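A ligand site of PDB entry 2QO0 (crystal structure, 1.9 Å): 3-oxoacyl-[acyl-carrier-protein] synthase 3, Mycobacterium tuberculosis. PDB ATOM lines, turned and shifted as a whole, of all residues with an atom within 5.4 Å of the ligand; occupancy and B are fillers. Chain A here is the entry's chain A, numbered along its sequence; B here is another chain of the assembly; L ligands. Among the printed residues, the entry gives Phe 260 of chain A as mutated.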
ATOM      1  N   ASN A  91       7.101  -8.711 -19.443  1.00  0.00           N
ATOM      2  CA  ASN A  91       6.732  -9.696 -20.450  1.00  0.00           C
ATOM      3  C   ASN A  91       7.134 -11.108 -20.007  1.00  0.00           C
ATOM      4  O   ASN A  91       6.916 -12.077 -20.730  1.00  0.00           O
ATOM      5  CB  ASN A  91       7.451  -9.410 -21.772  1.00  0.00           C
ATOM      6  CG  ASN A  91       7.085  -8.077 -22.346  1.00  0.00           C
ATOM      7  OD1 ASN A  91       6.087  -7.948 -23.038  1.00  0.00           O
ATOM      8  ND2 ASN A  91       7.900  -7.066 -22.074  1.00  0.00           N
ATOM      9  N   THR A  92       7.733 -11.209 -18.830  1.00  0.00           N
ATOM     10  CA  THR A  92       8.318 -12.475 -18.408  1.00  0.00           C
ATOM     11  C   THR A  92       7.886 -12.919 -17.022  1.00  0.00           C
ATOM     12  O   THR A  92       8.650 -13.529 -16.295  1.00  0.00           O
ATOM     13  CB  THR A  92       9.851 -12.479 -18.513  1.00  0.00           C
ATOM     14  OG1 THR A  92      10.363 -11.336 -17.838  1.00  0.00           O
ATOM     15  CG2 THR A  92      10.279 -12.459 -19.981  1.00  0.00           C
ATOM     16  N   PHE A  94       5.967 -15.699 -15.825  1.00  0.00           N
ATOM     17  CA  PHE A  94       5.529 -16.912 -16.516  1.00  0.00           C
ATOM     18  C   PHE A  94       4.384 -17.631 -15.835  1.00  0.00           C
ATOM     19  O   PHE A  94       4.351 -18.862 -15.792  1.00  0.00           O
ATOM     20  CB  PHE A  94       6.701 -17.871 -16.765  1.00  0.00           C
ATOM     21  CG  PHE A  94       7.884 -17.226 -17.427  1.00  0.00           C
ATOM     22  CD1 PHE A  94       9.067 -17.055 -16.718  1.00  0.00           C
ATOM     23  CD2 PHE A  94       7.822 -16.797 -18.759  1.00  0.00           C
ATOM     24  CE1 PHE A  94      10.179 -16.471 -17.314  1.00  0.00           C
ATOM     25  CE2 PHE A  94       8.928 -16.214 -19.377  1.00  0.00           C
ATOM     26  CZ  PHE A  94      10.118 -16.043 -18.647  1.00  0.00           C
ATOM     27  N   GLY A 121       4.588  -5.000 -24.387  1.00  0.00           N
ATOM     28  CA  GLY A 121       5.883  -5.322 -24.958  1.00  0.00           C
ATOM     29  C   GLY A 121       6.968  -4.537 -24.259  1.00  0.00           C
ATOM     30  O   GLY A 121       6.968  -4.412 -23.042  1.00  0.00           O
ATOM     31  N   CYS A 122       7.886  -3.983 -25.055  1.00  0.00           N
ATOM     32  CA  CYS A 122       8.979  -3.188 -24.504  1.00  0.00           C
ATOM     33  C   CYS A 122       8.502  -1.841 -23.958  1.00  0.00           C
ATOM     34  O   CYS A 122       9.086  -1.318 -23.011  1.00  0.00           O
ATOM     35  CB  CYS A 122      10.053  -2.964 -25.581  1.00  0.00           C
ATOM     36  SG  CYS A 122      11.091  -4.405 -25.960  1.00  0.00           S
ATOM     37  N   LEU A 152      14.360 -12.535 -19.236  1.00  0.00           N
ATOM     38  CA  LEU A 152      14.220 -12.906 -20.634  1.00  0.00           C
ATOM     39  C   LEU A 152      15.113 -14.100 -20.991  1.00  0.00           C
ATOM     40  O   LEU A 152      14.832 -14.832 -21.936  1.00  0.00           O
ATOM     41  CB  LEU A 152      14.573 -11.710 -21.517  1.00  0.00           C
ATOM     42  CG  LEU A 152      13.545 -10.593 -21.601  1.00  0.00           C
ATOM     43  CD1 LEU A 152      14.189  -9.256 -21.966  1.00  0.00           C
ATOM     44  CD2 LEU A 152      12.467 -10.961 -22.596  1.00  0.00           C
ATOM     45  N   THR A 155      13.832 -17.425 -22.289  1.00  0.00           N
ATOM     46  CA  THR A 155      12.994 -17.365 -23.495  1.00  0.00           C
ATOM     47  C   THR A 155      13.803 -17.390 -24.803  1.00  0.00           C
ATOM     48  O   THR A 155      13.239 -17.402 -25.907  1.00  0.00           O
ATOM     49  CB  THR A 155      12.092 -16.115 -23.474  1.00  0.00           C
ATOM     50  OG1 THR A 155      12.872 -14.953 -23.782  1.00  0.00           O
ATOM     51  CG2 THR A 155      11.427 -15.944 -22.124  1.00  0.00           C
ATOM     52  N   PHE A 167      18.488 -10.005 -25.909  1.00  0.00           N
ATOM     53  CA  PHE A 167      17.731  -9.863 -24.660  1.00  0.00           C
ATOM     54  C   PHE A 167      18.507 -10.225 -23.379  1.00  0.00           C
ATOM     55  O   PHE A 167      19.488 -10.972 -23.431  1.00  0.00           O
ATOM     56  CB  PHE A 167      16.410 -10.626 -24.735  1.00  0.00           C
ATOM     57  CG  PHE A 167      15.503 -10.147 -25.830  1.00  0.00           C
ATOM     58  CD1 PHE A 167      15.373 -10.866 -27.018  1.00  0.00           C
ATOM     59  CD2 PHE A 167      14.807  -8.948 -25.704  1.00  0.00           C
ATOM     60  CE1 PHE A 167      14.547 -10.411 -28.046  1.00  0.00           C
ATOM     61  CE2 PHE A 167      13.985  -8.482 -26.723  1.00  0.00           C
ATOM     62  CZ  PHE A 167      13.858  -9.212 -27.898  1.00  0.00           C
ATOM     63  N   ILE A 199       7.828  -8.992 -33.406  1.00  0.00           N
ATOM     64  CA  ILE A 199       8.492  -9.509 -32.198  1.00  0.00           C
ATOM     65  C   ILE A 199       7.452 -10.329 -31.457  1.00  0.00           C
ATOM     66  O   ILE A 199       6.396  -9.811 -31.095  1.00  0.00           O
ATOM     67  CB  ILE A 199       9.020  -8.390 -31.269  1.00  0.00           C
ATOM     68  CG1 ILE A 199      10.099  -7.554 -31.952  1.00  0.00           C
ATOM     69  CG2 ILE A 199       9.619  -8.988 -29.998  1.00  0.00           C
ATOM     70  CD1 ILE A 199      10.106  -6.114 -31.508  1.00  0.00           C
ATOM     71  N   ARG A 200       7.750 -11.611 -31.233  1.00  0.00           N
ATOM     72  CA  ARG A 200       6.756 -12.538 -30.711  1.00  0.00           C
ATOM     73  C   ARG A 200       7.344 -13.763 -29.993  1.00  0.00           C
ATOM     74  O   ARG A 200       8.486 -14.162 -30.236  1.00  0.00           O
ATOM     75  CB  ARG A 200       5.863 -13.030 -31.871  1.00  0.00           C
ATOM     76  CG  ARG A 200       6.517 -14.117 -32.718  1.00  0.00           C
ATOM     77  CD  ARG A 200       5.773 -14.342 -34.043  1.00  0.00           C
ATOM     78  NE  ARG A 200       6.484 -15.306 -34.884  1.00  0.00           N
ATOM     79  CZ  ARG A 200       7.592 -15.029 -35.586  1.00  0.00           C
ATOM     80  NH1 ARG A 200       8.133 -13.814 -35.551  1.00  0.00           N
ATOM     81  NH2 ARG A 200       8.163 -15.978 -36.310  1.00  0.00           N
ATOM     82  N   GLN A 201       6.531 -14.327 -29.099  1.00  0.00           N
ATOM     83  CA  GLN A 201       6.662 -15.722 -28.721  1.00  0.00           C
ATOM     84  C   GLN A 201       6.059 -16.523 -29.877  1.00  0.00           C
ATOM     85  O   GLN A 201       4.944 -16.204 -30.340  1.00  0.00           O
ATOM     86  CB  GLN A 201       5.900 -15.989 -27.418  1.00  0.00           C
ATOM     87  CG  GLN A 201       5.819 -17.442 -27.037  1.00  0.00           C
ATOM     88  CD  GLN A 201       5.106 -17.652 -25.721  1.00  0.00           C
ATOM     89  OE1 GLN A 201       5.212 -16.836 -24.807  1.00  0.00           O
ATOM     90  NE2 GLN A 201       4.381 -18.763 -25.614  1.00  0.00           N
ATOM     91  N   TRP A 205       1.449 -20.910 -25.303  1.00  0.00           N
ATOM     92  CA  TRP A 205       1.700 -21.892 -24.241  1.00  0.00           C
ATOM     93  C   TRP A 205       0.747 -23.077 -24.211  1.00  0.00           C
ATOM     94  O   TRP A 205       1.146 -24.190 -23.890  1.00  0.00           O
ATOM     95  CB  TRP A 205       1.672 -21.200 -22.883  1.00  0.00           C
ATOM     96  CG  TRP A 205       2.788 -20.271 -22.617  1.00  0.00           C
ATOM     97  CD1 TRP A 205       2.698 -18.933 -22.382  1.00  0.00           C
ATOM     98  CD2 TRP A 205       4.177 -20.613 -22.479  1.00  0.00           C
ATOM     99  NE1 TRP A 205       3.946 -18.415 -22.120  1.00  0.00           N
ATOM    100  CE2 TRP A 205       4.868 -19.423 -22.178  1.00  0.00           C
ATOM    101  CE3 TRP A 205       4.900 -21.805 -22.592  1.00  0.00           C
ATOM    102  CZ2 TRP A 205       6.246 -19.383 -21.992  1.00  0.00           C
ATOM    103  CZ3 TRP A 205       6.272 -21.768 -22.398  1.00  0.00           C
ATOM    104  CH2 TRP A 205       6.929 -20.566 -22.110  1.00  0.00           C
ATOM    105  N   ARG A 216       9.317 -26.370 -28.024  1.00  0.00           N
ATOM    106  CA  ARG A 216       8.931 -25.417 -27.003  1.00  0.00           C
ATOM    107  C   ARG A 216       8.982 -23.994 -27.572  1.00  0.00           C
ATOM    108  O   ARG A 216       9.683 -23.771 -28.574  1.00  0.00           O
ATOM    109  CB  ARG A 216       9.858 -25.523 -25.789  1.00  0.00           C
ATOM    110  CG  ARG A 216      11.329 -25.251 -26.082  1.00  0.00           C
ATOM    111  CD  ARG A 216      12.006 -24.645 -24.864  1.00  0.00           C
ATOM    112  NE  ARG A 216      11.678 -23.227 -24.696  1.00  0.00           N
ATOM    113  CZ  ARG A 216      12.157 -22.468 -23.708  1.00  0.00           C
ATOM    114  NH1 ARG A 216      12.975 -23.005 -22.824  1.00  0.00           N
ATOM    115  NH2 ARG A 216      11.830 -21.190 -23.612  1.00  0.00           N
ATOM    116  N   PRO A 217       8.250 -23.042 -26.960  1.00  0.00           N
ATOM    117  CA  PRO A 217       8.248 -21.647 -27.432  1.00  0.00           C
ATOM    118  C   PRO A 217       9.530 -20.896 -27.080  1.00  0.00           C
ATOM    119  O   PRO A 217      10.164 -21.189 -26.067  1.00  0.00           O
ATOM    120  CB  PRO A 217       7.044 -21.018 -26.700  1.00  0.00           C
ATOM    121  CG  PRO A 217       6.299 -22.173 -26.079  1.00  0.00           C
ATOM    122  CD  PRO A 217       7.342 -23.210 -25.815  1.00  0.00           C
ATOM    123  N   PHE A 218       9.892 -19.942 -27.940  1.00  0.00           N
ATOM    124  CA  PHE A 218      11.046 -19.055 -27.756  1.00  0.00           C
ATOM    125  C   PHE A 218      10.741 -17.681 -28.341  1.00  0.00           C
ATOM    126  O   PHE A 218       9.826 -17.523 -29.144  1.00  0.00           O
ATOM    127  CB  PHE A 218      12.245 -19.598 -28.514  1.00  0.00           C
ATOM    128  CG  PHE A 218      12.958 -20.745 -27.846  1.00  0.00           C
ATOM    129  CD1 PHE A 218      13.712 -20.540 -26.694  1.00  0.00           C
ATOM    130  CD2 PHE A 218      12.941 -22.006 -28.412  1.00  0.00           C
ATOM    131  CE1 PHE A 218      14.404 -21.592 -26.093  1.00  0.00           C
ATOM    132  CE2 PHE A 218      13.635 -23.066 -27.826  1.00  0.00           C
ATOM    133  CZ  PHE A 218      14.364 -22.849 -26.665  1.00  0.00           C
ATOM    134  N   VAL A 219      11.534 -16.675 -27.990  1.00  0.00           N
ATOM    135  CA  VAL A 219      11.376 -15.363 -28.633  1.00  0.00           C
ATOM    136  C   VAL A 219      11.884 -15.361 -30.090  1.00  0.00           C
ATOM    137  O   VAL A 219      12.950 -15.913 -30.399  1.00  0.00           O
ATOM    138  CB  VAL A 219      12.047 -14.240 -27.798  1.00  0.00           C
ATOM    139  CG1 VAL A 219      13.557 -14.390 -27.798  1.00  0.00           C
ATOM    140  CG2 VAL A 219      11.610 -12.852 -28.316  1.00  0.00           C
ATOM    141  N   HIS A 258      14.615   3.344 -25.837  1.00  0.00           N
ATOM    142  CA  HIS A 258      14.676   1.958 -25.464  1.00  0.00           C
ATOM    143  C   HIS A 258      16.008   1.373 -25.951  1.00  0.00           C
ATOM    144  O   HIS A 258      16.431   1.619 -27.096  1.00  0.00           O
ATOM    145  CB  HIS A 258      13.503   1.183 -26.040  1.00  0.00           C
ATOM    146  CG  HIS A 258      13.407  -0.188 -25.494  1.00  0.00           C
ATOM    147  ND1 HIS A 258      12.871  -0.460 -24.251  1.00  0.00           N
ATOM    148  CD2 HIS A 258      13.837  -1.367 -25.985  1.00  0.00           C
ATOM    149  CE1 HIS A 258      12.943  -1.753 -24.017  1.00  0.00           C
ATOM    150  NE2 HIS A 258      13.522  -2.335 -25.056  1.00  0.00           N
ATOM    151  N   PHE A 260      17.340  -1.082 -27.348  1.00  0.00           N
ATOM    152  CA  PHE A 260      16.993  -2.193 -28.214  1.00  0.00           C
ATOM    153  C   PHE A 260      18.132  -2.511 -29.167  1.00  0.00           C
ATOM    154  O   PHE A 260      18.484  -3.673 -29.378  1.00  0.00           O
ATOM    155  CB  PHE A 260      15.750  -1.820 -29.040  1.00  0.00           C
ATOM    156  CG  PHE A 260      14.950  -3.006 -29.502  1.00  0.00           C
ATOM    157  CD1 PHE A 260      13.648  -3.190 -29.051  1.00  0.00           C
ATOM    158  CD2 PHE A 260      15.489  -3.937 -30.380  1.00  0.00           C
ATOM    159  CE1 PHE A 260      12.888  -4.272 -29.475  1.00  0.00           C
ATOM    160  CE2 PHE A 260      14.732  -5.029 -30.805  1.00  0.00           C
ATOM    161  CZ  PHE A 260      13.433  -5.202 -30.345  1.00  0.00           C
ATOM    162  N   SER A 291      13.966  -5.217 -22.257  1.00  0.00           N
ATOM    163  CA  SER A 291      12.546  -4.933 -22.536  1.00  0.00           C
ATOM    164  C   SER A 291      11.956  -3.891 -21.574  1.00  0.00           C
ATOM    165  O   SER A 291      12.498  -2.804 -21.432  1.00  0.00           O
ATOM    166  CB  SER A 291      11.723  -6.216 -22.582  1.00  0.00           C
ATOM    167  OG  SER A 291      10.393  -5.970 -23.008  1.00  0.00           O
ATOM    168  N   TYR A 319       9.817   1.509 -27.112  1.00  0.00           N
ATOM    169  CA  TYR A 319       9.333   0.927 -28.365  1.00  0.00           C
ATOM    170  C   TYR A 319       9.674  -0.559 -28.463  1.00  0.00           C
ATOM    171  O   TYR A 319      10.719  -0.985 -27.996  1.00  0.00           O
ATOM    172  CB  TYR A 319       9.858   1.699 -29.581  1.00  0.00           C
ATOM    173  CG  TYR A 319      11.372   1.662 -29.732  1.00  0.00           C
ATOM    174  CD1 TYR A 319      12.000   0.649 -30.471  1.00  0.00           C
ATOM    175  CD2 TYR A 319      12.170   2.634 -29.158  1.00  0.00           C
ATOM    176  CE1 TYR A 319      13.384   0.599 -30.593  1.00  0.00           C
ATOM    177  CE2 TYR A 319      13.555   2.608 -29.299  1.00  0.00           C
ATOM    178  CZ  TYR A 319      14.154   1.592 -30.009  1.00  0.00           C
ATOM    179  OH  TYR A 319      15.531   1.563 -30.143  1.00  0.00           O
ATOM    180  N   GLY A 320       8.793  -1.341 -29.079  1.00  0.00           N
ATOM    181  CA  GLY A 320       9.062  -2.757 -29.246  1.00  0.00           C
ATOM    182  C   GLY A 320       7.825  -3.557 -29.589  1.00  0.00           C
ATOM    183  O   GLY A 320       6.970  -3.079 -30.344  1.00  0.00           O
ATOM    184  N   ALA A 321       7.745  -4.748 -29.009  1.00  0.00           N
ATOM    185  CA  ALA A 321       6.761  -5.783 -29.367  1.00  0.00           C
ATOM    186  C   ALA A 321       5.322  -5.350 -29.237  1.00  0.00           C
ATOM    187  O   ALA A 321       4.991  -4.458 -28.452  1.00  0.00           O
ATOM    188  CB  ALA A 321       6.989  -7.051 -28.535  1.00  0.00           C
ATOM    189  N   GLN B  96       3.607 -14.502 -24.031  1.00  0.00           N
ATOM    190  CA  GLN B  96       4.335 -13.539 -23.208  1.00  0.00           C
ATOM    191  C   GLN B  96       4.419 -12.186 -23.906  1.00  0.00           C
ATOM    192  O   GLN B  96       4.313 -11.129 -23.283  1.00  0.00           O
ATOM    193  CB  GLN B  96       5.743 -14.045 -22.875  1.00  0.00           C
ATOM    194  CG  GLN B  96       5.766 -15.345 -22.066  1.00  0.00           C
ATOM    195  CD  GLN B  96       5.032 -15.278 -20.741  1.00  0.00           C
ATOM    196  OE1 GLN B  96       4.309 -16.206 -20.379  1.00  0.00           O
ATOM    197  NE2 GLN B  96       5.214 -14.173 -20.009  1.00  0.00           N
ATOM    198  N   THR B  97       4.616 -12.246 -25.224  1.00  0.00           N
ATOM    199  CA  THR B  97       4.513 -11.108 -26.136  1.00  0.00           C
ATOM    200  C   THR B  97       4.187 -11.687 -27.526  1.00  0.00           C
ATOM    201  O   THR B  97       4.464 -12.869 -27.774  1.00  0.00           O
ATOM    202  CB  THR B  97       5.819 -10.245 -26.149  1.00  0.00           C
ATOM    203  OG1 THR B  97       5.477  -8.858 -26.212  1.00  0.00           O
ATOM    204  CG2 THR B  97       6.754 -10.604 -27.317  1.00  0.00           C
HETATM  205  C1  LIG L   1       9.114 -17.833 -24.830  1.00  0.00           C
HETATM  206  C2  LIG L   1       8.555 -16.410 -24.708  1.00  0.00           C
HETATM  207  C3  LIG L   1       9.229 -15.447 -25.699  1.00  0.00           C
HETATM  208  C4  LIG L   1       8.748 -13.993 -25.532  1.00  0.00           C
HETATM  209  C5  LIG L   1       9.499 -13.235 -24.426  1.00  0.00           C
HETATM  210  C6  LIG L   1       8.984 -11.785 -24.323  1.00  0.00           C
HETATM  211  C7  LIG L   1       9.695 -10.893 -25.322  1.00  0.00           C
HETATM  212  C8  LIG L   1       9.653  -9.412 -24.909  1.00  0.00           C
HETATM  213  C9  LIG L   1      10.120  -8.487 -26.057  1.00  0.00           C
HETATM  214  C10 LIG L   1       9.443  -7.119 -25.869  1.00  0.00           C
HETATM  215  S1  LIG L   1      10.112  -5.828 -26.973  1.00  0.00           S
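S1 of the ligand is covalently linked to SG of Cys 122.
The backbone NH of Cys 122 sits close to a sulfur (S1) of the ligand.
The backbone NH of Ala 321 sits close to a sulfur (S1) of the ligand (3.3 Å).
O of Leu 152 is in hydrogen-bond range of OG1 of Thr 155, 2.7 Å away.
The backbone carbonyl oxygen (O) of Thr 155 sits at hydrogen-bond distance from the backbone NH (N) of Val 219 (2.8 Å).
The side-chain amide nitrogen (ND2) of Asn 91 lies within hydrogen-bond range of the side-chain hydroxyl (OG) of Ser 291.
The backbone carbonyl oxygen of Gly 121 is in hydrogen-bond range of the side-chain amide nitrogen of Asn 91, at 3.0 Å.
OE1 of Gln 96 of chain B is in hydrogen-bond range of NE1 of Trp 205, 2.8 Å away.
The side-chain sulfur (SG) of Cys 122 is in hydrogen-bond range of a ring nitrogen (NE2) of His 258 (3.3 Å).
The backbone NH (N) of Gln 201 lies within hydrogen-bond range of the backbone carbonyl oxygen (O) of Thr 97 of chain B (2.9 Å).
The side-chain amide oxygen (OE1) of Gln 201 lies within hydrogen-bond range of the indole nitrogen (NE1) of Trp 205, at 3.4 Å.
Residues that only touch the ligand: Ser 291 (3.2 Å), Gln 201 (3.4 Å), Val 219 (3.5 Å), Thr 97 of chain B (3.6 Å), Thr 155 (3.7 Å), Phe 218 (3.7 Å), Pro 217 (3.7 Å), Asn 91 (3.8 Å), Leu 152 (3.9 Å), Phe 167 (3.9 Å), Gly 121 (3.9 Å), Gly 320 (3.96 Å) and Gln 96 of chain B (3.99 Å).
Hydrophobic or aromatic side chains that line the ligand: Leu 152, Phe 167, Val 219 and Ala 321.
The nearest printed residue that does not touch the ligand is Ile 199 (4.004 Å).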
